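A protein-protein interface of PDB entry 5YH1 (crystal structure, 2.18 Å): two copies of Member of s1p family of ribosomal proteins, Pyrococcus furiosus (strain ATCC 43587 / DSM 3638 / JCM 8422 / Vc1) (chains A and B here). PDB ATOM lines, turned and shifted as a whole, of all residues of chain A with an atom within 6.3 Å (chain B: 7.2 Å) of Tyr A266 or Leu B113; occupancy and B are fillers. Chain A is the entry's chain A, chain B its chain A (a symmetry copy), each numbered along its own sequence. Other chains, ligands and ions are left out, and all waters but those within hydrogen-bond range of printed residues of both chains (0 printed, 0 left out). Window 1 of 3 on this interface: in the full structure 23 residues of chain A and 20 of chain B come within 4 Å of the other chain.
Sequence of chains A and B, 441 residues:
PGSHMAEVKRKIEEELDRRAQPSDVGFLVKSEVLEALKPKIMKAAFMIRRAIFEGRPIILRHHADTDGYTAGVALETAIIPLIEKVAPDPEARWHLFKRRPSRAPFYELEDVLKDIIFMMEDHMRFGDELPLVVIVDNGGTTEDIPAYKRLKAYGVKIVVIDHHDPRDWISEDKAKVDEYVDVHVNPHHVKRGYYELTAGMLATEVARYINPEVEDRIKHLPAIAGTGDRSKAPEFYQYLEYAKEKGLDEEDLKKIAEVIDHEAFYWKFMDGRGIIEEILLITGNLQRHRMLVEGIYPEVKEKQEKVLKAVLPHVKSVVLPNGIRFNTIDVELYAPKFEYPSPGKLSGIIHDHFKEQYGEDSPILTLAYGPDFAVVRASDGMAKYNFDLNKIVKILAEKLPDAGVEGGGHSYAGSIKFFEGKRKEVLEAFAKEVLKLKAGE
Tyr A266 touches three residues of chain B.
Printed residues of chain B within 4 Å of Glu A299: Leu B109 and Arg B150.
Printed residues of chain A within 4 Å of Leu B109: His A262, Tyr A266 and Glu A299.
Leu B113 touches just these residues of chain A: Glu A263 (3.5 Å), Tyr A266 (3.7 Å) and Ile A275 (3.9 Å).
Of the printed residues of chain A, Ile B116 touches Ile A275.
The nearest residue of chain B that does not touch Tyr A266 is Asp B111 (6.0 Å).
No position is printed for both chains.
Among the printed residues, merely in contact across the chains: Met A270 with Phe B118 (3.3 Å), Glu A263 with Leu B113 (3.5 Å), Tyr A266 with Glu B110 (3.5 Å), His A262 with Arg B150 (3.6 Å), His A262 with Leu B109 (3.6 Å), Met A270 with Ile B117 (3.6 Å), Ile A275 with Ile B116 (3.6 Å), Glu A299 with Leu B109 (3.6 Å), Lys A268 with Glu B110 (3.7 Å), Met A270 with Lys B114 (3.7 Å), Tyr A266 with Leu B113 (3.7 Å), Tyr A266 with Leu B109 (3.8 Å), Ile A275 with Ile B117 (3.8 Å) and Ile A275 with Leu B113 (3.9 Å).
Hydrophobic or aromatic side chains of chain A within 4 Å of the printed part of chain B: His A262, Tyr A266, Met A270 and Ile A275.
Of the 17 printed residues of chain B, 8 touch a printed residue of chain A.
Hydrophobic or aromatic side chains of chain B within 4 Å of the printed part of chain A: Leu B109, Leu B113, Ile B116, Ile B117 and Phe B118.
Along chain B the printed residues that touch a printed residue of chain A span positions 109 to 150.
Among the printed residues, Asp or Glu carboxylates within 4 Å of a Lys or Arg side-chain nitrogen of the other chain: Glu A263 with Arg B150 (2.7 Å) and Glu A299 with Arg B150 (2.9 Å).
OE1 of Glu A263 sits at hydrogen-bond distance from ND1 of His A262 (2.7 Å).
A ring nitrogen (NE2) of His A262 is in hydrogen-bond range of the side-chain amino group (NZ) of Lys A303 (3.1 Å).
The side-chain amino group (NZ) of Lys A303 is in hydrogen-bond range of the side-chain hydroxyl (OH) of Tyr A266.
NE1 of Trp A267 lies close to O of Met A270 (3.4 Å).
The guanidinium group (NE) of Arg B150 is in salt-bridge range of the side-chain carboxylate (OE2) of Glu A263 (2.7 Å).
OE2 of Glu A299 is in salt-bridge range of NH2 of Arg B150.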
ATOM      1  N   ASP A 261     -14.274 -14.131 -31.596  1.00  0.00           N
ATOM      2  CA  ASP A 261     -15.628 -13.696 -31.240  1.00  0.00           C
ATOM      3  C   ASP A 261     -15.836 -13.667 -29.715  1.00  0.00           C
ATOM      4  O   ASP A 261     -16.600 -12.846 -29.208  1.00  0.00           O
ATOM      5  CB  ASP A 261     -16.693 -14.582 -31.901  1.00  0.00           C
ATOM      6  CG  ASP A 261     -16.725 -14.444 -33.430  1.00  0.00           C
ATOM      7  OD1 ASP A 261     -16.300 -13.406 -33.982  1.00  0.00           O
ATOM      8  OD2 ASP A 261     -17.192 -15.385 -34.091  1.00  0.00           O
ATOM      9  N   HIS A 262     -15.155 -14.564 -29.000  1.00  0.00           N
ATOM     10  CA  HIS A 262     -15.226 -14.613 -27.542  1.00  0.00           C
ATOM     11  C   HIS A 262     -14.460 -13.433 -26.940  1.00  0.00           C
ATOM     12  O   HIS A 262     -15.030 -12.629 -26.218  1.00  0.00           O
ATOM     13  CB  HIS A 262     -14.676 -15.950 -27.029  1.00  0.00           C
ATOM     14  CG  HIS A 262     -14.628 -16.062 -25.541  1.00  0.00           C
ATOM     15  ND1 HIS A 262     -13.549 -15.636 -24.796  1.00  0.00           N
ATOM     16  CD2 HIS A 262     -15.514 -16.580 -24.658  1.00  0.00           C
ATOM     17  CE1 HIS A 262     -13.777 -15.880 -23.518  1.00  0.00           C
ATOM     18  NE2 HIS A 262     -14.963 -16.449 -23.409  1.00  0.00           N
ATOM     19  N   GLU A 263     -13.179 -13.316 -27.269  1.00  0.00           N
ATOM     20  CA  GLU A 263     -12.379 -12.208 -26.761  1.00  0.00           C
ATOM     21  C   GLU A 263     -12.980 -10.835 -27.111  1.00  0.00           C
ATOM     22  O   GLU A 263     -13.001  -9.933 -26.266  1.00  0.00           O
ATOM     23  CB  GLU A 263     -10.917 -12.297 -27.233  1.00  0.00           C
ATOM     24  CG  GLU A 263     -10.177 -13.555 -26.793  1.00  0.00           C
ATOM     25  CD  GLU A 263     -10.205 -13.792 -25.287  1.00  0.00           C
ATOM     26  OE1 GLU A 263     -11.092 -14.536 -24.809  1.00  0.00           O
ATOM     27  OE2 GLU A 263      -9.332 -13.246 -24.579  1.00  0.00           O
ATOM     28  N   ALA A 264     -13.467 -10.671 -28.338  1.00  0.00           N
ATOM     29  CA  ALA A 264     -14.020  -9.374 -28.762  1.00  0.00           C
ATOM     30  C   ALA A 264     -15.292  -8.999 -28.000  1.00  0.00           C
ATOM     31  O   ALA A 264     -15.591  -7.820 -27.836  1.00  0.00           O
ATOM     32  CB  ALA A 264     -14.281  -9.351 -30.262  1.00  0.00           C
ATOM     33  N   PHE A 265     -16.048  -9.999 -27.570  1.00  0.00           N
ATOM     34  CA  PHE A 265     -17.191  -9.776 -26.695  1.00  0.00           C
ATOM     35  C   PHE A 265     -16.758  -9.068 -25.406  1.00  0.00           C
ATOM     36  O   PHE A 265     -17.434  -8.158 -24.938  1.00  0.00           O
ATOM     37  CB  PHE A 265     -17.885 -11.113 -26.373  1.00  0.00           C
ATOM     38  CG  PHE A 265     -19.025 -10.989 -25.396  1.00  0.00           C
ATOM     39  CD1 PHE A 265     -20.315 -10.739 -25.843  1.00  0.00           C
ATOM     40  CD2 PHE A 265     -18.806 -11.128 -24.027  1.00  0.00           C
ATOM     41  CE1 PHE A 265     -21.367 -10.625 -24.943  1.00  0.00           C
ATOM     42  CE2 PHE A 265     -19.851 -10.999 -23.123  1.00  0.00           C
ATOM     43  CZ  PHE A 265     -21.132 -10.749 -23.581  1.00  0.00           C
ATOM     44  N   TYR A 266     -15.622  -9.477 -24.850  1.00  0.00           N
ATOM     45  CA  TYR A 266     -15.161  -8.933 -23.579  1.00  0.00           C
ATOM     46  C   TYR A 266     -14.381  -7.623 -23.697  1.00  0.00           C
ATOM     47  O   TYR A 266     -14.459  -6.793 -22.794  1.00  0.00           O
ATOM     48  CB  TYR A 266     -14.353  -9.974 -22.801  1.00  0.00           C
ATOM     49  CG  TYR A 266     -15.206 -11.101 -22.266  1.00  0.00           C
ATOM     50  CD1 TYR A 266     -15.970 -10.945 -21.101  1.00  0.00           C
ATOM     51  CD2 TYR A 266     -15.265 -12.319 -22.927  1.00  0.00           C
ATOM     52  CE1 TYR A 266     -16.755 -11.984 -20.614  1.00  0.00           C
ATOM     53  CE2 TYR A 266     -16.041 -13.360 -22.442  1.00  0.00           C
ATOM     54  CZ  TYR A 266     -16.779 -13.194 -21.291  1.00  0.00           C
ATOM     55  OH  TYR A 266     -17.539 -14.250 -20.839  1.00  0.00           O
ATOM     56  N   TRP A 267     -13.636  -7.412 -24.780  1.00  0.00           N
ATOM     57  CA  TRP A 267     -12.927  -6.146 -24.909  1.00  0.00           C
ATOM     58  C   TRP A 267     -13.782  -5.039 -25.548  1.00  0.00           C
ATOM     59  O   TRP A 267     -13.359  -3.897 -25.585  1.00  0.00           O
ATOM     60  CB  TRP A 267     -11.544  -6.304 -25.568  1.00  0.00           C
ATOM     61  CG  TRP A 267     -11.477  -6.610 -27.031  1.00  0.00           C
ATOM     62  CD1 TRP A 267     -12.145  -5.980 -28.035  1.00  0.00           C
ATOM     63  CD2 TRP A 267     -10.617  -7.573 -27.667  1.00  0.00           C
ATOM     64  NE1 TRP A 267     -11.795  -6.522 -29.257  1.00  0.00           N
ATOM     65  CE2 TRP A 267     -10.857  -7.498 -29.060  1.00  0.00           C
ATOM     66  CE3 TRP A 267      -9.681  -8.498 -27.196  1.00  0.00           C
ATOM     67  CZ2 TRP A 267     -10.204  -8.321 -29.982  1.00  0.00           C
ATOM     68  CZ3 TRP A 267      -9.026  -9.315 -28.121  1.00  0.00           C
ATOM     69  CH2 TRP A 267      -9.296  -9.221 -29.493  1.00  0.00           C
ATOM     70  N   LYS A 268     -14.958  -5.400 -26.068  1.00  0.00           N
ATOM     71  CA  LYS A 268     -16.022  -4.446 -26.435  1.00  0.00           C
ATOM     72  C   LYS A 268     -15.602  -3.350 -27.446  1.00  0.00           C
ATOM     73  O   LYS A 268     -15.381  -3.638 -28.623  1.00  0.00           O
ATOM     74  CB  LYS A 268     -16.619  -3.819 -25.162  1.00  0.00           C
ATOM     75  CG  LYS A 268     -17.565  -4.727 -24.388  1.00  0.00           C
ATOM     76  CD  LYS A 268     -17.945  -4.127 -23.033  1.00  0.00           C
ATOM     77  CE  LYS A 268     -18.796  -2.860 -23.142  1.00  0.00           C
ATOM     78  NZ  LYS A 268     -20.266  -3.124 -23.137  1.00  0.00           N
ATOM     79  N   MET A 270     -12.860  -1.534 -27.376  1.00  0.00           N
ATOM     80  CA  MET A 270     -11.418  -1.561 -27.638  1.00  0.00           C
ATOM     81  C   MET A 270     -11.164  -2.365 -28.889  1.00  0.00           C
ATOM     82  O   MET A 270     -12.016  -3.127 -29.324  1.00  0.00           O
ATOM     83  CB  MET A 270     -10.673  -2.135 -26.436  1.00  0.00           C
ATOM     84  CG  MET A 270     -10.934  -1.284 -25.190  1.00  0.00           C
ATOM     85  SD  MET A 270      -9.797  -1.929 -23.706  1.00  0.00           S
ATOM     86  CE  MET A 270      -8.204  -0.957 -24.300  1.00  0.00           C
ATOM     87  N   ILE A 275      -3.206  -8.122 -29.287  1.00  0.00           N
ATOM     88  CA  ILE A 275      -3.783  -9.449 -29.081  1.00  0.00           C
ATOM     89  C   ILE A 275      -4.296 -10.038 -30.400  1.00  0.00           C
ATOM     90  O   ILE A 275      -3.944 -11.161 -30.753  1.00  0.00           O
ATOM     91  CB  ILE A 275      -4.935  -9.417 -28.057  1.00  0.00           C
ATOM     92  CG1 ILE A 275      -4.506  -8.641 -26.801  1.00  0.00           C
ATOM     93  CG2 ILE A 275      -5.359 -10.833 -27.682  1.00  0.00           C
ATOM     94  CD1 ILE A 275      -5.584  -8.506 -25.745  1.00  0.00           C
ATOM     95  N   GLU A 299     -11.749 -23.040 -22.862  1.00  0.00           N
ATOM     96  CA  GLU A 299     -12.619 -22.211 -22.038  1.00  0.00           C
ATOM     97  C   GLU A 299     -13.865 -21.808 -22.823  1.00  0.00           C
ATOM     98  O   GLU A 299     -14.976 -21.905 -22.320  1.00  0.00           O
ATOM     99  CB  GLU A 299     -11.784 -21.012 -21.571  1.00  0.00           C
ATOM    100  CG  GLU A 299     -12.479 -19.801 -20.996  1.00  0.00           C
ATOM    101  CD  GLU A 299     -11.468 -18.702 -20.685  1.00  0.00           C
ATOM    102  OE1 GLU A 299     -10.280 -19.024 -20.395  1.00  0.00           O
ATOM    103  OE2 GLU A 299     -11.848 -17.515 -20.759  1.00  0.00           O
ATOM    104  N   LYS A 303     -17.782 -23.124 -22.052  1.00  0.00           N
ATOM    105  CA  LYS A 303     -18.916 -22.208 -21.868  1.00  0.00           C
ATOM    106  C   LYS A 303     -20.073 -22.545 -22.791  1.00  0.00           C
ATOM    107  O   LYS A 303     -21.223 -22.569 -22.367  1.00  0.00           O
ATOM    108  CB  LYS A 303     -18.520 -20.764 -22.133  1.00  0.00           C
ATOM    109  CG  LYS A 303     -17.661 -20.138 -21.061  1.00  0.00           C
ATOM    110  CD  LYS A 303     -17.390 -18.690 -21.424  1.00  0.00           C
ATOM    111  CE  LYS A 303     -16.388 -18.076 -20.476  1.00  0.00           C
ATOM    112  NZ  LYS A 303     -16.288 -16.602 -20.653  1.00  0.00           N
ATOM    113  N   GLU A 339     -24.156 -12.114 -20.192  1.00  0.00           N
ATOM    114  CA  GLU A 339     -22.949 -12.930 -20.209  1.00  0.00           C
ATOM    115  C   GLU A 339     -22.716 -13.509 -21.587  1.00  0.00           C
ATOM    116  O   GLU A 339     -23.627 -13.573 -22.401  1.00  0.00           O
ATOM    117  CB  GLU A 339     -23.071 -14.076 -19.217  1.00  0.00           C
ATOM    118  CG  GLU A 339     -23.065 -13.650 -17.763  1.00  0.00           C
ATOM    119  CD  GLU A 339     -23.319 -14.823 -16.843  1.00  0.00           C
ATOM    120  OE1 GLU A 339     -22.684 -15.882 -17.038  1.00  0.00           O
ATOM    121  OE2 GLU A 339     -24.163 -14.696 -15.938  1.00  0.00           O
ATOM    122  N   TYR A 340     -21.485 -13.931 -21.845  1.00  0.00           N
ATOM    123  CA  TYR A 340     -21.205 -14.727 -23.022  1.00  0.00           C
ATOM    124  C   TYR A 340     -21.934 -16.063 -22.857  1.00  0.00           C
ATOM    125  O   TYR A 340     -21.816 -16.691 -21.819  1.00  0.00           O
ATOM    126  CB  TYR A 340     -19.710 -14.964 -23.176  1.00  0.00           C
ATOM    127  CG  TYR A 340     -19.362 -15.819 -24.365  1.00  0.00           C
ATOM    128  CD1 TYR A 340     -19.328 -17.201 -24.256  1.00  0.00           C
ATOM    129  CD2 TYR A 340     -19.086 -15.247 -25.606  1.00  0.00           C
ATOM    130  CE1 TYR A 340     -19.019 -17.996 -25.343  1.00  0.00           C
ATOM    131  CE2 TYR A 340     -18.771 -16.035 -26.700  1.00  0.00           C
ATOM    132  CZ  TYR A 340     -18.742 -17.413 -26.562  1.00  0.00           C
ATOM    133  OH  TYR A 340     -18.438 -18.220 -27.636  1.00  0.00           O
ATOM    134  N   ARG B  61      -4.114  -4.024  -9.587  1.00  0.00           N
ATOM    135  CA  ARG B  61      -5.564  -4.222  -9.613  1.00  0.00           C
ATOM    136  C   ARG B  61      -6.037  -4.566  -8.218  1.00  0.00           C
ATOM    137  O   ARG B  61      -5.424  -5.408  -7.553  1.00  0.00           O
ATOM    138  CB  ARG B  61      -5.922  -5.393 -10.518  1.00  0.00           C
ATOM    139  CG  ARG B  61      -5.912  -5.077 -11.994  1.00  0.00           C
ATOM    140  CD  ARG B  61      -7.315  -4.768 -12.466  1.00  0.00           C
ATOM    141  NE  ARG B  61      -7.320  -4.211 -13.813  1.00  0.00           N
ATOM    142  CZ  ARG B  61      -8.287  -3.434 -14.289  1.00  0.00           C
ATOM    143  NH1 ARG B  61      -9.338  -3.125 -13.536  1.00  0.00           N
ATOM    144  NH2 ARG B  61      -8.211  -2.975 -15.525  1.00  0.00           N
ATOM    145  N   TYR B 107     -10.679 -11.283 -11.287  1.00  0.00           N
ATOM    146  CA  TYR B 107     -10.004 -10.581 -12.366  1.00  0.00           C
ATOM    147  C   TYR B 107     -10.762 -10.870 -13.674  1.00  0.00           C
ATOM    148  O   TYR B 107     -10.486 -11.843 -14.367  1.00  0.00           O
ATOM    149  CB  TYR B 107      -8.539 -11.031 -12.413  1.00  0.00           C
ATOM    150  CG  TYR B 107      -7.555 -10.146 -13.158  1.00  0.00           C
ATOM    151  CD1 TYR B 107      -7.933  -8.941 -13.752  1.00  0.00           C
ATOM    152  CD2 TYR B 107      -6.219 -10.517 -13.243  1.00  0.00           C
ATOM    153  CE1 TYR B 107      -7.006  -8.154 -14.425  1.00  0.00           C
ATOM    154  CE2 TYR B 107      -5.291  -9.730 -13.900  1.00  0.00           C
ATOM    155  CZ  TYR B 107      -5.687  -8.549 -14.487  1.00  0.00           C
ATOM    156  OH  TYR B 107      -4.746  -7.775 -15.139  1.00  0.00           O
ATOM    157  N   GLU B 108     -11.754 -10.033 -13.958  1.00  0.00           N
ATOM    158  CA  GLU B 108     -12.630 -10.159 -15.131  1.00  0.00           C
ATOM    159  C   GLU B 108     -11.877 -10.071 -16.430  1.00  0.00           C
ATOM    160  O   GLU B 108     -10.897  -9.339 -16.513  1.00  0.00           O
ATOM    161  CB  GLU B 108     -13.607  -8.993 -15.174  1.00  0.00           C
ATOM    162  CG  GLU B 108     -14.888  -9.194 -14.437  1.00  0.00           C
ATOM    163  CD  GLU B 108     -15.812  -8.019 -14.654  1.00  0.00           C
ATOM    164  OE1 GLU B 108     -16.913  -8.231 -15.185  1.00  0.00           O
ATOM    165  OE2 GLU B 108     -15.422  -6.888 -14.323  1.00  0.00           O
ATOM    166  N   LEU B 109     -12.391 -10.724 -17.470  1.00  0.00           N
ATOM    167  CA  LEU B 109     -11.735 -10.673 -18.785  1.00  0.00           C
ATOM    168  C   LEU B 109     -11.697  -9.260 -19.347  1.00  0.00           C
ATOM    169  O   LEU B 109     -10.708  -8.871 -19.965  1.00  0.00           O
ATOM    170  CB  LEU B 109     -12.378 -11.633 -19.788  1.00  0.00           C
ATOM    171  CG  LEU B 109     -12.166 -13.126 -19.513  1.00  0.00           C
ATOM    172  CD1 LEU B 109     -12.673 -13.965 -20.673  1.00  0.00           C
ATOM    173  CD2 LEU B 109     -10.704 -13.440 -19.244  1.00  0.00           C
ATOM    174  N   GLU B 110     -12.748  -8.478 -19.110  1.00  0.00           N
ATOM    175  CA  GLU B 110     -12.756  -7.097 -19.577  1.00  0.00           C
ATOM    176  C   GLU B 110     -11.601  -6.306 -18.955  1.00  0.00           C
ATOM    177  O   GLU B 110     -10.982  -5.485 -19.631  1.00  0.00           O
ATOM    178  CB  GLU B 110     -14.103  -6.420 -19.289  1.00  0.00           C
ATOM    179  CG  GLU B 110     -14.172  -4.992 -19.817  1.00  0.00           C
ATOM    180  CD  GLU B 110     -15.580  -4.400 -19.834  1.00  0.00           C
ATOM    181  OE1 GLU B 110     -16.550  -5.094 -19.462  1.00  0.00           O
ATOM    182  OE2 GLU B 110     -15.718  -3.223 -20.236  1.00  0.00           O
ATOM    183  N   ASP B 111     -11.305  -6.561 -17.677  1.00  0.00           N
ATOM    184  CA  ASP B 111     -10.182  -5.908 -17.004  1.00  0.00           C
ATOM    185  C   ASP B 111      -8.832  -6.359 -17.548  1.00  0.00           C
ATOM    186  O   ASP B 111      -7.996  -5.529 -17.880  1.00  0.00           O
ATOM    187  CB  ASP B 111     -10.216  -6.154 -15.488  1.00  0.00           C
ATOM    188  CG  ASP B 111     -11.391  -5.463 -14.805  1.00  0.00           C
ATOM    189  OD1 ASP B 111     -12.084  -4.662 -15.455  1.00  0.00           O
ATOM    190  OD2 ASP B 111     -11.632  -5.734 -13.613  1.00  0.00           O
ATOM    191  N   VAL B 112      -8.602  -7.669 -17.617  1.00  0.00           N
ATOM    192  CA  VAL B 112      -7.292  -8.150 -18.044  1.00  0.00           C
ATOM    193  C   VAL B 112      -7.029  -7.824 -19.522  1.00  0.00           C
ATOM    194  O   VAL B 112      -5.900  -7.494 -19.909  1.00  0.00           O
ATOM    195  CB  VAL B 112      -7.102  -9.651 -17.756  1.00  0.00           C
ATOM    196  CG1 VAL B 112      -7.931 -10.516 -18.699  1.00  0.00           C
ATOM    197  CG2 VAL B 112      -5.630 -10.005 -17.842  1.00  0.00           C
ATOM    198  N   LEU B 113      -8.068  -7.868 -20.345  1.00  0.00           N
ATOM    199  CA  LEU B 113      -7.874  -7.583 -21.775  1.00  0.00           C
ATOM    200  C   LEU B 113      -7.501  -6.121 -21.975  1.00  0.00           C
ATOM    201  O   LEU B 113      -6.640  -5.793 -22.785  1.00  0.00           O
ATOM    202  CB  LEU B 113      -9.108  -7.990 -22.586  1.00  0.00           C
ATOM    203  CG  LEU B 113      -9.293  -9.519 -22.645  1.00  0.00           C
ATOM    204  CD1 LEU B 113     -10.636  -9.874 -23.249  1.00  0.00           C
ATOM    205  CD2 LEU B 113      -8.166 -10.187 -23.417  1.00  0.00           C
ATOM    206  N   LYS B 114      -8.125  -5.246 -21.201  1.00  0.00           N
ATOM    207  CA  LYS B 114      -7.753  -3.843 -21.205  1.00  0.00           C
ATOM    208  C   LYS B 114      -6.289  -3.667 -20.734  1.00  0.00           C
ATOM    209  O   LYS B 114      -5.505  -2.945 -21.352  1.00  0.00           O
ATOM    210  CB  LYS B 114      -8.747  -3.066 -20.333  1.00  0.00           C
ATOM    211  CG  LYS B 114      -8.508  -1.573 -20.248  1.00  0.00           C
ATOM    212  CD  LYS B 114      -7.806  -1.198 -18.961  1.00  0.00           C
ATOM    213  CE  LYS B 114      -7.651   0.309 -18.830  1.00  0.00           C
ATOM    214  NZ  LYS B 114      -8.822   0.918 -18.140  1.00  0.00           N
ATOM    215  N   ASP B 115      -5.918  -4.351 -19.660  1.00  0.00           N
ATOM    216  CA  ASP B 115      -4.546  -4.284 -19.158  1.00  0.00           C
ATOM    217  C   ASP B 115      -3.532  -4.739 -20.230  1.00  0.00           C
ATOM    218  O   ASP B 115      -2.476  -4.135 -20.409  1.00  0.00           O
ATOM    219  CB  ASP B 115      -4.407  -5.145 -17.880  1.00  0.00           C
ATOM    220  CG  ASP B 115      -5.175  -4.566 -16.687  1.00  0.00           C
ATOM    221  OD1 ASP B 115      -5.552  -3.376 -16.736  1.00  0.00           O
ATOM    222  OD2 ASP B 115      -5.403  -5.303 -15.700  1.00  0.00           O
ATOM    223  N   ILE B 116      -3.860  -5.803 -20.948  1.00  0.00           N
ATOM    224  CA  ILE B 116      -2.972  -6.316 -21.992  1.00  0.00           C
ATOM    225  C   ILE B 116      -2.882  -5.338 -23.181  1.00  0.00           C
ATOM    226  O   ILE B 116      -1.797  -5.055 -23.683  1.00  0.00           O
ATOM    227  CB  ILE B 116      -3.398  -7.736 -22.439  1.00  0.00           C
ATOM    228  CG1 ILE B 116      -3.148  -8.724 -21.295  1.00  0.00           C
ATOM    229  CG2 ILE B 116      -2.620  -8.191 -23.684  1.00  0.00           C
ATOM    230  CD1 ILE B 116      -3.800 -10.083 -21.479  1.00  0.00           C
ATOM    231  N   ILE B 117      -4.006  -4.791 -23.618  1.00  0.00           N
ATOM    232  CA  ILE B 117      -3.986  -3.847 -24.748  1.00  0.00           C
ATOM    233  C   ILE B 117      -3.177  -2.608 -24.380  1.00  0.00           C
ATOM    234  O   ILE B 117      -2.326  -2.164 -25.147  1.00  0.00           O
ATOM    235  CB  ILE B 117      -5.416  -3.477 -25.193  1.00  0.00           C
ATOM    236  CG1 ILE B 117      -6.084  -4.701 -25.826  1.00  0.00           C
ATOM    237  CG2 ILE B 117      -5.413  -2.289 -26.165  1.00  0.00           C
ATOM    238  CD1 ILE B 117      -7.597  -4.680 -25.797  1.00  0.00           C
ATOM    239  N   PHE B 118      -3.422  -2.067 -23.192  1.00  0.00           N
ATOM    240  CA  PHE B 118      -2.700  -0.891 -22.714  1.00  0.00           C
ATOM    241  C   PHE B 118      -1.205  -1.166 -22.563  1.00  0.00           C
ATOM    242  O   PHE B 118      -0.389  -0.357 -22.984  1.00  0.00           O
ATOM    243  CB  PHE B 118      -3.290  -0.396 -21.382  1.00  0.00           C
ATOM    244  CG  PHE B 118      -4.463   0.544 -21.532  1.00  0.00           C
ATOM    245  CD1 PHE B 118      -5.379   0.417 -22.579  1.00  0.00           C
ATOM    246  CD2 PHE B 118      -4.665   1.560 -20.602  1.00  0.00           C
ATOM    247  CE1 PHE B 118      -6.458   1.292 -22.696  1.00  0.00           C
ATOM    248  CE2 PHE B 118      -5.744   2.436 -20.716  1.00  0.00           C
ATOM    249  CZ  PHE B 118      -6.639   2.301 -21.769  1.00  0.00           C
ATOM    250  N   MET B 119      -0.836  -2.296 -21.963  1.00  0.00           N
ATOM    251  CA  MET B 119       0.595  -2.599 -21.759  1.00  0.00           C
ATOM    252  C   MET B 119       1.294  -2.841 -23.086  1.00  0.00           C
ATOM    253  O   MET B 119       2.457  -2.478 -23.248  1.00  0.00           O
ATOM    254  CB  MET B 119       0.808  -3.762 -20.777  1.00  0.00           C
ATOM    255  CG  MET B 119       0.563  -5.119 -21.428  1.00  0.00           C
ATOM    256  SD  MET B 119       0.771  -6.679 -20.232  1.00  0.00           S
ATOM    257  CE  MET B 119      -0.604  -6.298 -18.876  1.00  0.00           C
ATOM    258  N   ALA B 147      -7.818 -15.154 -16.669  1.00  0.00           N
ATOM    259  CA  ALA B 147      -7.023 -13.933 -16.812  1.00  0.00           C
ATOM    260  C   ALA B 147      -5.535 -14.234 -16.815  1.00  0.00           C
ATOM    261  O   ALA B 147      -4.770 -13.644 -17.582  1.00  0.00           O
ATOM    262  CB  ALA B 147      -7.356 -12.951 -15.693  1.00  0.00           C
ATOM    263  N   ARG B 150      -4.099 -15.721 -20.024  1.00  0.00           N
ATOM    264  CA  ARG B 150      -3.859 -14.678 -21.000  1.00  0.00           C
ATOM    265  C   ARG B 150      -2.598 -13.886 -20.699  1.00  0.00           C
ATOM    266  O   ARG B 150      -1.792 -13.646 -21.606  1.00  0.00           O
ATOM    267  CB  ARG B 150      -5.077 -13.769 -21.123  1.00  0.00           C
ATOM    268  CG  ARG B 150      -6.226 -14.459 -21.839  1.00  0.00           C
ATOM    269  CD  ARG B 150      -7.533 -13.770 -21.541  1.00  0.00           C
ATOM    270  NE  ARG B 150      -8.670 -14.370 -22.233  1.00  0.00           N
ATOM    271  CZ  ARG B 150      -9.280 -15.491 -21.865  1.00  0.00           C
ATOM    272  NH1 ARG B 150      -8.857 -16.194 -20.812  1.00  0.00           N
ATOM    273  NH2 ARG B 150     -10.324 -15.919 -22.566  1.00  0.00           N
ATOM    274  N   LEU B 151      -2.395 -13.505 -19.436  1.00  0.00           N
ATOM    275  CA  LEU B 151      -1.158 -12.804 -19.065  1.00  0.00           C
ATOM    276  C   LEU B 151       0.103 -13.649 -19.319  1.00  0.00           C
ATOM    277  O   LEU B 151       1.150 -13.119 -19.706  1.00  0.00           O
ATOM    278  CB  LEU B 151      -1.203 -12.332 -17.605  1.00  0.00           C
ATOM    279  CG  LEU B 151      -2.183 -11.190 -17.324  1.00  0.00           C
ATOM    280  CD1 LEU B 151      -2.359 -10.991 -15.829  1.00  0.00           C
ATOM    281  CD2 LEU B 151      -1.726  -9.895 -17.973  1.00  0.00           C
